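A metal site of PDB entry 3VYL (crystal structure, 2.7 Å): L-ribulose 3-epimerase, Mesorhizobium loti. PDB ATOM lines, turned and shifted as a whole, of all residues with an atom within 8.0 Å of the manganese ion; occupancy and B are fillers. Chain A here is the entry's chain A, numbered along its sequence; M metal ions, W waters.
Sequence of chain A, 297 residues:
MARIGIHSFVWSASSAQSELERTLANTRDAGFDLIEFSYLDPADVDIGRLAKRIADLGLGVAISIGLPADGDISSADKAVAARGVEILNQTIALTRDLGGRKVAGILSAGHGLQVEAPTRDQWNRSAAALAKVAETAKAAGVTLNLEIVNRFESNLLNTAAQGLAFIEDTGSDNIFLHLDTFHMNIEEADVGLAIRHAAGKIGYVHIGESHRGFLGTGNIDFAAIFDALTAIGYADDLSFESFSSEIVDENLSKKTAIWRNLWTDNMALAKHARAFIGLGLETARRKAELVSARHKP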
ATOM      1  N   HIS A   7      20.486  34.285  15.692  1.00  0.00           N
ATOM      2  CA  HIS A   7      19.237  34.242  16.441  1.00  0.00           C
ATOM      3  C   HIS A   7      18.380  35.443  16.104  1.00  0.00           C
ATOM      4  O   HIS A   7      18.879  36.568  16.073  1.00  0.00           O
ATOM      5  CB  HIS A   7      19.520  34.215  17.930  1.00  0.00           C
ATOM      6  CG  HIS A   7      18.357  33.741  18.761  1.00  0.00           C
ATOM      7  ND1 HIS A   7      18.403  32.603  19.480  1.00  0.00           N
ATOM      8  CD2 HIS A   7      17.085  34.276  18.952  1.00  0.00           C
ATOM      9  CE1 HIS A   7      17.222  32.429  20.107  1.00  0.00           C
ATOM     10  NE2 HIS A   7      16.417  33.457  19.774  1.00  0.00           N
ATOM     11  N   GLU A  36      17.260  31.500  13.469  1.00  0.00           N
ATOM     12  CA  GLU A  36      16.749  30.815  14.635  1.00  0.00           C
ATOM     13  C   GLU A  36      15.641  31.651  15.278  1.00  0.00           C
ATOM     14  O   GLU A  36      15.830  32.830  15.600  1.00  0.00           O
ATOM     15  CB  GLU A  36      17.887  30.570  15.626  1.00  0.00           C
ATOM     16  CG  GLU A  36      17.538  29.790  16.888  1.00  0.00           C
ATOM     17  CD  GLU A  36      18.768  29.451  17.699  1.00  0.00           C
ATOM     18  OE1 GLU A  36      19.873  29.594  17.132  1.00  0.00           O
ATOM     19  OE2 GLU A  36      18.667  29.060  18.882  1.00  0.00           O
ATOM     20  N   SER A  64      14.521  27.363  18.883  1.00  0.00           N
ATOM     21  CA  SER A  64      15.030  27.152  20.224  1.00  0.00           C
ATOM     22  C   SER A  64      14.061  27.770  21.191  1.00  0.00           C
ATOM     23  O   SER A  64      13.521  28.838  20.935  1.00  0.00           O
ATOM     24  CB  SER A  64      16.385  27.835  20.382  1.00  0.00           C
ATOM     25  OG  SER A  64      16.248  29.241  20.321  1.00  0.00           O
ATOM     26  N   GLY A 105      17.614  24.491  22.395  1.00  0.00           N
ATOM     27  CA  GLY A 105      17.328  25.279  23.558  1.00  0.00           C
ATOM     28  C   GLY A 105      17.352  24.482  24.817  1.00  0.00           C
ATOM     29  O   GLY A 105      17.893  23.418  24.847  1.00  0.00           O
ATOM     30  N   ILE A 106      16.784  25.033  25.867  1.00  0.00           N
ATOM     31  CA  ILE A 106      16.732  24.333  27.125  1.00  0.00           C
ATOM     32  C   ILE A 106      15.483  23.529  27.159  1.00  0.00           C
ATOM     33  O   ILE A 106      14.425  24.018  27.295  1.00  0.00           O
ATOM     34  CB  ILE A 106      16.748  25.313  28.296  1.00  0.00           C
ATOM     35  CG1 ILE A 106      17.745  26.411  28.040  1.00  0.00           C
ATOM     36  CG2 ILE A 106      17.164  24.624  29.561  1.00  0.00           C
ATOM     37  CD1 ILE A 106      18.169  27.054  29.316  1.00  0.00           C
ATOM     38  N   GLU A 147      20.244  21.999  24.930  1.00  0.00           N
ATOM     39  CA  GLU A 147      21.205  23.062  25.246  1.00  0.00           C
ATOM     40  C   GLU A 147      21.772  22.895  26.628  1.00  0.00           C
ATOM     41  O   GLU A 147      21.036  22.681  27.609  1.00  0.00           O
ATOM     42  CB  GLU A 147      20.701  24.497  25.042  1.00  0.00           C
ATOM     43  CG  GLU A 147      21.852  25.502  24.917  1.00  0.00           C
ATOM     44  CD  GLU A 147      21.455  26.944  24.604  1.00  0.00           C
ATOM     45  OE1 GLU A 147      20.271  27.225  24.387  1.00  0.00           O
ATOM     46  OE2 GLU A 147      22.353  27.810  24.574  1.00  0.00           O
ATOM     47  N   ILE A 148      23.090  22.957  26.680  1.00  0.00           N
ATOM     48  CA  ILE A 148      23.868  22.877  27.900  1.00  0.00           C
ATOM     49  C   ILE A 148      24.145  24.304  28.343  1.00  0.00           C
ATOM     50  O   ILE A 148      24.723  25.095  27.593  1.00  0.00           O
ATOM     51  CB  ILE A 148      25.201  22.158  27.620  1.00  0.00           C
ATOM     52  CG1 ILE A 148      24.935  20.824  26.926  1.00  0.00           C
ATOM     53  CG2 ILE A 148      26.005  21.986  28.904  1.00  0.00           C
ATOM     54  CD1 ILE A 148      24.107  19.822  27.714  1.00  0.00           C
ATOM     55  N   VAL A 149      23.726  24.635  29.562  1.00  0.00           N
ATOM     56  CA  VAL A 149      23.757  26.031  30.010  1.00  0.00           C
ATOM     57  C   VAL A 149      24.445  26.192  31.365  1.00  0.00           C
ATOM     58  O   VAL A 149      24.692  25.207  32.080  1.00  0.00           O
ATOM     59  CB  VAL A 149      22.350  26.688  30.023  1.00  0.00           C
ATOM     60  CG1 VAL A 149      21.778  26.728  28.618  1.00  0.00           C
ATOM     61  CG2 VAL A 149      21.410  25.970  30.959  1.00  0.00           C
ATOM     62  N   GLU A 153      21.177  29.344  34.764  1.00  0.00           N
ATOM     63  CA  GLU A 153      20.073  29.177  33.868  1.00  0.00           C
ATOM     64  C   GLU A 153      19.372  27.800  33.895  1.00  0.00           C
ATOM     65  O   GLU A 153      18.280  27.667  33.446  1.00  0.00           O
ATOM     66  CB  GLU A 153      20.498  29.606  32.495  1.00  0.00           C
ATOM     67  CG  GLU A 153      21.083  30.992  32.474  1.00  0.00           C
ATOM     68  CD  GLU A 153      21.046  31.627  31.129  1.00  0.00           C
ATOM     69  OE1 GLU A 153      20.202  31.260  30.355  1.00  0.00           O
ATOM     70  OE2 GLU A 153      21.841  32.472  30.807  1.00  0.00           O
ATOM     71  N   HIS A 178      23.396  20.526  22.223  1.00  0.00           N
ATOM     72  CA  HIS A 178      23.438  21.892  21.781  1.00  0.00           C
ATOM     73  C   HIS A 178      24.388  22.571  22.728  1.00  0.00           C
ATOM     74  O   HIS A 178      24.097  22.755  23.909  1.00  0.00           O
ATOM     75  CB  HIS A 178      22.037  22.497  21.828  1.00  0.00           C
ATOM     76  CG  HIS A 178      21.972  23.967  21.471  1.00  0.00           C
ATOM     77  ND1 HIS A 178      20.853  24.700  21.653  1.00  0.00           N
ATOM     78  CD2 HIS A 178      22.930  24.840  20.961  1.00  0.00           C
ATOM     79  CE1 HIS A 178      21.073  25.960  21.266  1.00  0.00           C
ATOM     80  NE2 HIS A 178      22.348  26.053  20.854  1.00  0.00           N
ATOM     81  N   LEU A 179      25.565  22.870  22.208  1.00  0.00           N
ATOM     82  CA  LEU A 179      26.610  23.549  22.972  1.00  0.00           C
ATOM     83  C   LEU A 179      26.630  25.070  22.700  1.00  0.00           C
ATOM     84  O   LEU A 179      26.357  25.527  21.570  1.00  0.00           O
ATOM     85  CB  LEU A 179      27.966  22.925  22.652  1.00  0.00           C
ATOM     86  CG  LEU A 179      28.155  21.432  22.957  1.00  0.00           C
ATOM     87  CD1 LEU A 179      29.576  21.019  22.633  1.00  0.00           C
ATOM     88  CD2 LEU A 179      27.833  21.084  24.398  1.00  0.00           C
ATOM     89  N   ASP A 180      26.952  25.856  23.724  1.00  0.00           N
ATOM     90  CA  ASP A 180      26.965  27.310  23.595  1.00  0.00           C
ATOM     91  C   ASP A 180      28.232  27.879  24.238  1.00  0.00           C
ATOM     92  O   ASP A 180      28.441  27.784  25.447  1.00  0.00           O
ATOM     93  CB  ASP A 180      25.679  27.875  24.233  1.00  0.00           C
ATOM     94  CG  ASP A 180      25.578  29.383  24.146  1.00  0.00           C
ATOM     95  OD1 ASP A 180      26.604  30.080  24.310  1.00  0.00           O
ATOM     96  OD2 ASP A 180      24.449  29.891  23.942  1.00  0.00           O
ATOM     97  N   THR A 181      29.092  28.488  23.418  1.00  0.00           N
ATOM     98  CA  THR A 181      30.388  28.960  23.872  1.00  0.00           C
ATOM     99  C   THR A 181      30.314  29.867  25.109  1.00  0.00           C
ATOM    100  O   THR A 181      31.116  29.727  26.037  1.00  0.00           O
ATOM    101  CB  THR A 181      31.148  29.647  22.740  1.00  0.00           C
ATOM    102  OG1 THR A 181      30.413  30.799  22.308  1.00  0.00           O
ATOM    103  CG2 THR A 181      31.326  28.707  21.550  1.00  0.00           C
ATOM    104  N   PHE A 182      29.324  30.757  25.146  1.00  0.00           N
ATOM    105  CA  PHE A 182      29.059  31.596  26.322  1.00  0.00           C
ATOM    106  C   PHE A 182      28.847  30.753  27.598  1.00  0.00           C
ATOM    107  O   PHE A 182      29.402  31.075  28.649  1.00  0.00           O
ATOM    108  CB  PHE A 182      27.867  32.525  26.063  1.00  0.00           C
ATOM    109  CG  PHE A 182      27.310  33.142  27.324  1.00  0.00           C
ATOM    110  CD1 PHE A 182      27.929  34.244  27.900  1.00  0.00           C
ATOM    111  CD2 PHE A 182      26.179  32.598  27.948  1.00  0.00           C
ATOM    112  CE1 PHE A 182      27.431  34.799  29.058  1.00  0.00           C
ATOM    113  CE2 PHE A 182      25.689  33.152  29.100  1.00  0.00           C
ATOM    114  CZ  PHE A 182      26.308  34.249  29.663  1.00  0.00           C
ATOM    115  N   HIS A 183      28.063  29.688  27.510  1.00  0.00           N
ATOM    116  CA  HIS A 183      27.849  28.809  28.657  1.00  0.00           C
ATOM    117  C   HIS A 183      29.027  27.928  28.965  1.00  0.00           C
ATOM    118  O   HIS A 183      29.351  27.675  30.139  1.00  0.00           O
ATOM    119  CB  HIS A 183      26.600  27.978  28.437  1.00  0.00           C
ATOM    120  CG  HIS A 183      25.342  28.801  28.325  1.00  0.00           C
ATOM    121  ND1 HIS A 183      24.823  29.465  29.376  1.00  0.00           N
ATOM    122  CD2 HIS A 183      24.523  29.076  27.244  1.00  0.00           C
ATOM    123  CE1 HIS A 183      23.718  30.132  28.982  1.00  0.00           C
ATOM    124  NE2 HIS A 183      23.533  29.885  27.677  1.00  0.00           N
ATOM    125  N   TYR A 204      24.093  21.001  17.432  1.00  0.00           N
ATOM    126  CA  TYR A 204      23.969  22.427  17.155  1.00  0.00           C
ATOM    127  C   TYR A 204      24.931  23.241  18.025  1.00  0.00           C
ATOM    128  O   TYR A 204      25.262  22.822  19.152  1.00  0.00           O
ATOM    129  CB  TYR A 204      22.513  22.847  17.391  1.00  0.00           C
ATOM    130  CG  TYR A 204      22.064  24.167  16.788  1.00  0.00           C
ATOM    131  CD1 TYR A 204      21.350  25.082  17.567  1.00  0.00           C
ATOM    132  CD2 TYR A 204      22.324  24.490  15.450  1.00  0.00           C
ATOM    133  CE1 TYR A 204      20.916  26.280  17.037  1.00  0.00           C
ATOM    134  CE2 TYR A 204      21.898  25.687  14.914  1.00  0.00           C
ATOM    135  CZ  TYR A 204      21.186  26.588  15.712  1.00  0.00           C
ATOM    136  OH  TYR A 204      20.751  27.796  15.210  1.00  0.00           O
ATOM    137  N   VAL A 205      25.382  24.384  17.527  1.00  0.00           N
ATOM    138  CA  VAL A 205      26.318  25.229  18.286  1.00  0.00           C
ATOM    139  C   VAL A 205      25.899  26.707  18.290  1.00  0.00           C
ATOM    140  O   VAL A 205      25.549  27.261  17.249  1.00  0.00           O
ATOM    141  CB  VAL A 205      27.774  25.101  17.759  1.00  0.00           C
ATOM    142  CG1 VAL A 205      28.654  26.217  18.308  1.00  0.00           C
ATOM    143  CG2 VAL A 205      28.345  23.740  18.114  1.00  0.00           C
ATOM    144  N   HIS A 206      25.949  27.331  19.469  1.00  0.00           N
ATOM    145  CA  HIS A 206      25.825  28.789  19.549  1.00  0.00           C
ATOM    146  C   HIS A 206      27.172  29.424  19.723  1.00  0.00           C
ATOM    147  O   HIS A 206      27.906  29.106  20.656  1.00  0.00           O
ATOM    148  CB  HIS A 206      24.940  29.200  20.714  1.00  0.00           C
ATOM    149  CG  HIS A 206      23.471  29.207  20.404  1.00  0.00           C
ATOM    150  ND1 HIS A 206      22.528  29.056  21.366  1.00  0.00           N
ATOM    151  CD2 HIS A 206      22.778  29.349  19.204  1.00  0.00           C
ATOM    152  CE1 HIS A 206      21.307  29.093  20.812  1.00  0.00           C
ATOM    153  NE2 HIS A 206      21.453  29.265  19.483  1.00  0.00           N
ATOM    154  N   ILE A 207      27.501  30.330  18.820  1.00  0.00           N
ATOM    155  CA  ILE A 207      28.663  31.183  18.982  1.00  0.00           C
ATOM    156  C   ILE A 207      28.235  32.476  19.696  1.00  0.00           C
ATOM    157  O   ILE A 207      27.405  33.217  19.201  1.00  0.00           O
ATOM    158  CB  ILE A 207      29.305  31.488  17.604  1.00  0.00           C
ATOM    159  CG1 ILE A 207      29.790  30.193  16.954  1.00  0.00           C
ATOM    160  CG2 ILE A 207      30.446  32.494  17.725  1.00  0.00           C
ATOM    161  CD1 ILE A 207      30.744  29.355  17.791  1.00  0.00           C
ATOM    162  N   GLY A 208      28.808  32.703  20.864  1.00  0.00           N
ATOM    163  CA  GLY A 208      28.526  33.910  21.639  1.00  0.00           C
ATOM    164  C   GLY A 208      29.737  34.243  22.483  1.00  0.00           C
ATOM    165  O   GLY A 208      30.372  33.352  23.020  1.00  0.00           O
ATOM    166  N   ARG A 212      28.526  38.122  25.935  1.00  0.00           N
ATOM    167  CA  ARG A 212      27.419  38.083  24.979  1.00  0.00           C
ATOM    168  C   ARG A 212      27.331  39.288  24.045  1.00  0.00           C
ATOM    169  O   ARG A 212      26.306  39.521  23.426  1.00  0.00           O
ATOM    170  CB  ARG A 212      26.078  37.825  25.701  1.00  0.00           C
ATOM    171  CG  ARG A 212      25.547  36.415  25.575  1.00  0.00           C
ATOM    172  CD  ARG A 212      24.731  36.034  26.806  1.00  0.00           C
ATOM    173  NE  ARG A 212      23.927  34.799  26.701  1.00  0.00           N
ATOM    174  CZ  ARG A 212      23.923  33.985  25.659  1.00  0.00           C
ATOM    175  NH1 ARG A 212      24.689  34.248  24.595  1.00  0.00           N
ATOM    176  NH2 ARG A 212      23.162  32.896  25.678  1.00  0.00           N
ATOM    177  N   SER A 239      25.179  28.993  15.116  1.00  0.00           N
ATOM    178  CA  SER A 239      24.608  30.332  15.025  1.00  0.00           C
ATOM    179  C   SER A 239      25.167  31.322  15.998  1.00  0.00           C
ATOM    180  O   SER A 239      25.518  30.969  17.119  1.00  0.00           O
ATOM    181  CB  SER A 239      23.101  30.283  15.169  1.00  0.00           C
ATOM    182  OG  SER A 239      22.565  29.725  13.992  1.00  0.00           O
ATOM    183  N   PHE A 240      25.232  32.571  15.546  1.00  0.00           N
ATOM    184  CA  PHE A 240      25.645  33.699  16.358  1.00  0.00           C
ATOM    185  C   PHE A 240      24.519  34.115  17.297  1.00  0.00           C
ATOM    186  O   PHE A 240      23.356  34.141  16.900  1.00  0.00           O
ATOM    187  CB  PHE A 240      26.034  34.854  15.439  1.00  0.00           C
ATOM    188  CG  PHE A 240      26.320  36.138  16.166  1.00  0.00           C
ATOM    189  CD1 PHE A 240      27.233  36.177  17.224  1.00  0.00           C
ATOM    190  CD2 PHE A 240      25.682  37.307  15.778  1.00  0.00           C
ATOM    191  CE1 PHE A 240      27.511  37.367  17.870  1.00  0.00           C
ATOM    192  CE2 PHE A 240      25.952  38.498  16.431  1.00  0.00           C
ATOM    193  CZ  PHE A 240      26.875  38.523  17.473  1.00  0.00           C
ATOM    194  N   GLU A 241      24.876  34.457  18.533  1.00  0.00           N
ATOM    195  CA  GLU A 241      23.905  34.775  19.591  1.00  0.00           C
ATOM    196  C   GLU A 241      24.421  35.987  20.393  1.00  0.00           C
ATOM    197  O   GLU A 241      25.549  36.004  20.863  1.00  0.00           O
ATOM    198  CB  GLU A 241      23.726  33.548  20.501  1.00  0.00           C
ATOM    199  CG  GLU A 241      22.450  33.487  21.330  1.00  0.00           C
ATOM    200  CD  GLU A 241      22.400  32.299  22.302  1.00  0.00           C
ATOM    201  OE1 GLU A 241      21.357  32.112  22.964  1.00  0.00           O
ATOM    202  OE2 GLU A 241      23.371  31.540  22.429  1.00  0.00           O
ATOM    203  N   PHE A 243      22.395  39.476  22.639  1.00  0.00           N
ATOM    204  CA  PHE A 243      21.115  40.122  22.903  1.00  0.00           C
ATOM    205  C   PHE A 243      21.241  41.546  23.451  1.00  0.00           C
ATOM    206  O   PHE A 243      22.300  41.917  24.010  1.00  0.00           O
ATOM    207  CB  PHE A 243      20.228  39.231  23.784  1.00  0.00           C
ATOM    208  CG  PHE A 243      19.989  37.851  23.221  1.00  0.00           C
ATOM    209  CD1 PHE A 243      19.460  37.670  21.926  1.00  0.00           C
ATOM    210  CD2 PHE A 243      20.255  36.717  23.989  1.00  0.00           C
ATOM    211  CE1 PHE A 243      19.228  36.398  21.423  1.00  0.00           C
ATOM    212  CE2 PHE A 243      20.017  35.433  23.482  1.00  0.00           C
ATOM    213  CZ  PHE A 243      19.499  35.281  22.208  1.00  0.00           C
HETATM  214 MN    MN M   1      22.466  29.601  23.468  1.00  0.00          MN
HETATM  215  O   HOH W   1      20.966  30.525  25.063  1.00  0.00           O
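Water W1 lies within hydrogen-bond range of OE1 of Glu 241, NH2 of Arg 212 and OE1 of Glu 147.
Four residues have an atom within 4 Å of the manganese ion: Glu 147, Asp 180, His 206 and Glu 241.
The nearest printed residue that does not touch the manganese ion is Arg 212 (4.03 Å).
N of Thr 181 lies within hydrogen-bond range of O of His 206.
A ring nitrogen (ND1) of His 206 lies close to a ring nitrogen (NE2) of His 178, at 3.1 Å.
The backbone NH (N) of Glu 241 sits at hydrogen-bond distance from the backbone carbonyl oxygen (O) of Ile 207 (2.9 Å).
The side-chain carboxylate of Asp 180 sits close to the guanidinium group of Arg 212, 3.7 Å away.
The side-chain carboxylate (OD1) of Asp 180 is in hydrogen-bond range of the backbone NH (N) of Phe 182 (2.9 Å).
A ring nitrogen (NE2) of His 206 is in hydrogen-bond range of the side-chain carboxylate (OE1) of Glu 36, at 2.9 Å.
The backbone NH of His 206 is in hydrogen-bond range of the backbone carbonyl oxygen of Leu 179, at 2.8 Å.
The side-chain carboxylate (OE1) of Glu 241 is in salt-bridge range of the guanidinium group (NH2) of Arg 212 (3.4 Å).
The manganese ion is bound by the side-chain carboxylate (OD2) of Asp 180 (2.1 Å), the side-chain carboxylate (OE2) of Glu 147 (2.1 Å), a ring nitrogen (ND1) of His 206 (2.2 Å), water W1 (2.4 Å) and the side-chain carboxylate (OE2) of Glu 241 (2.4 Å).
Slightly farther from the manganese ion lies OE1 of Glu 241 (2.8 Å).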
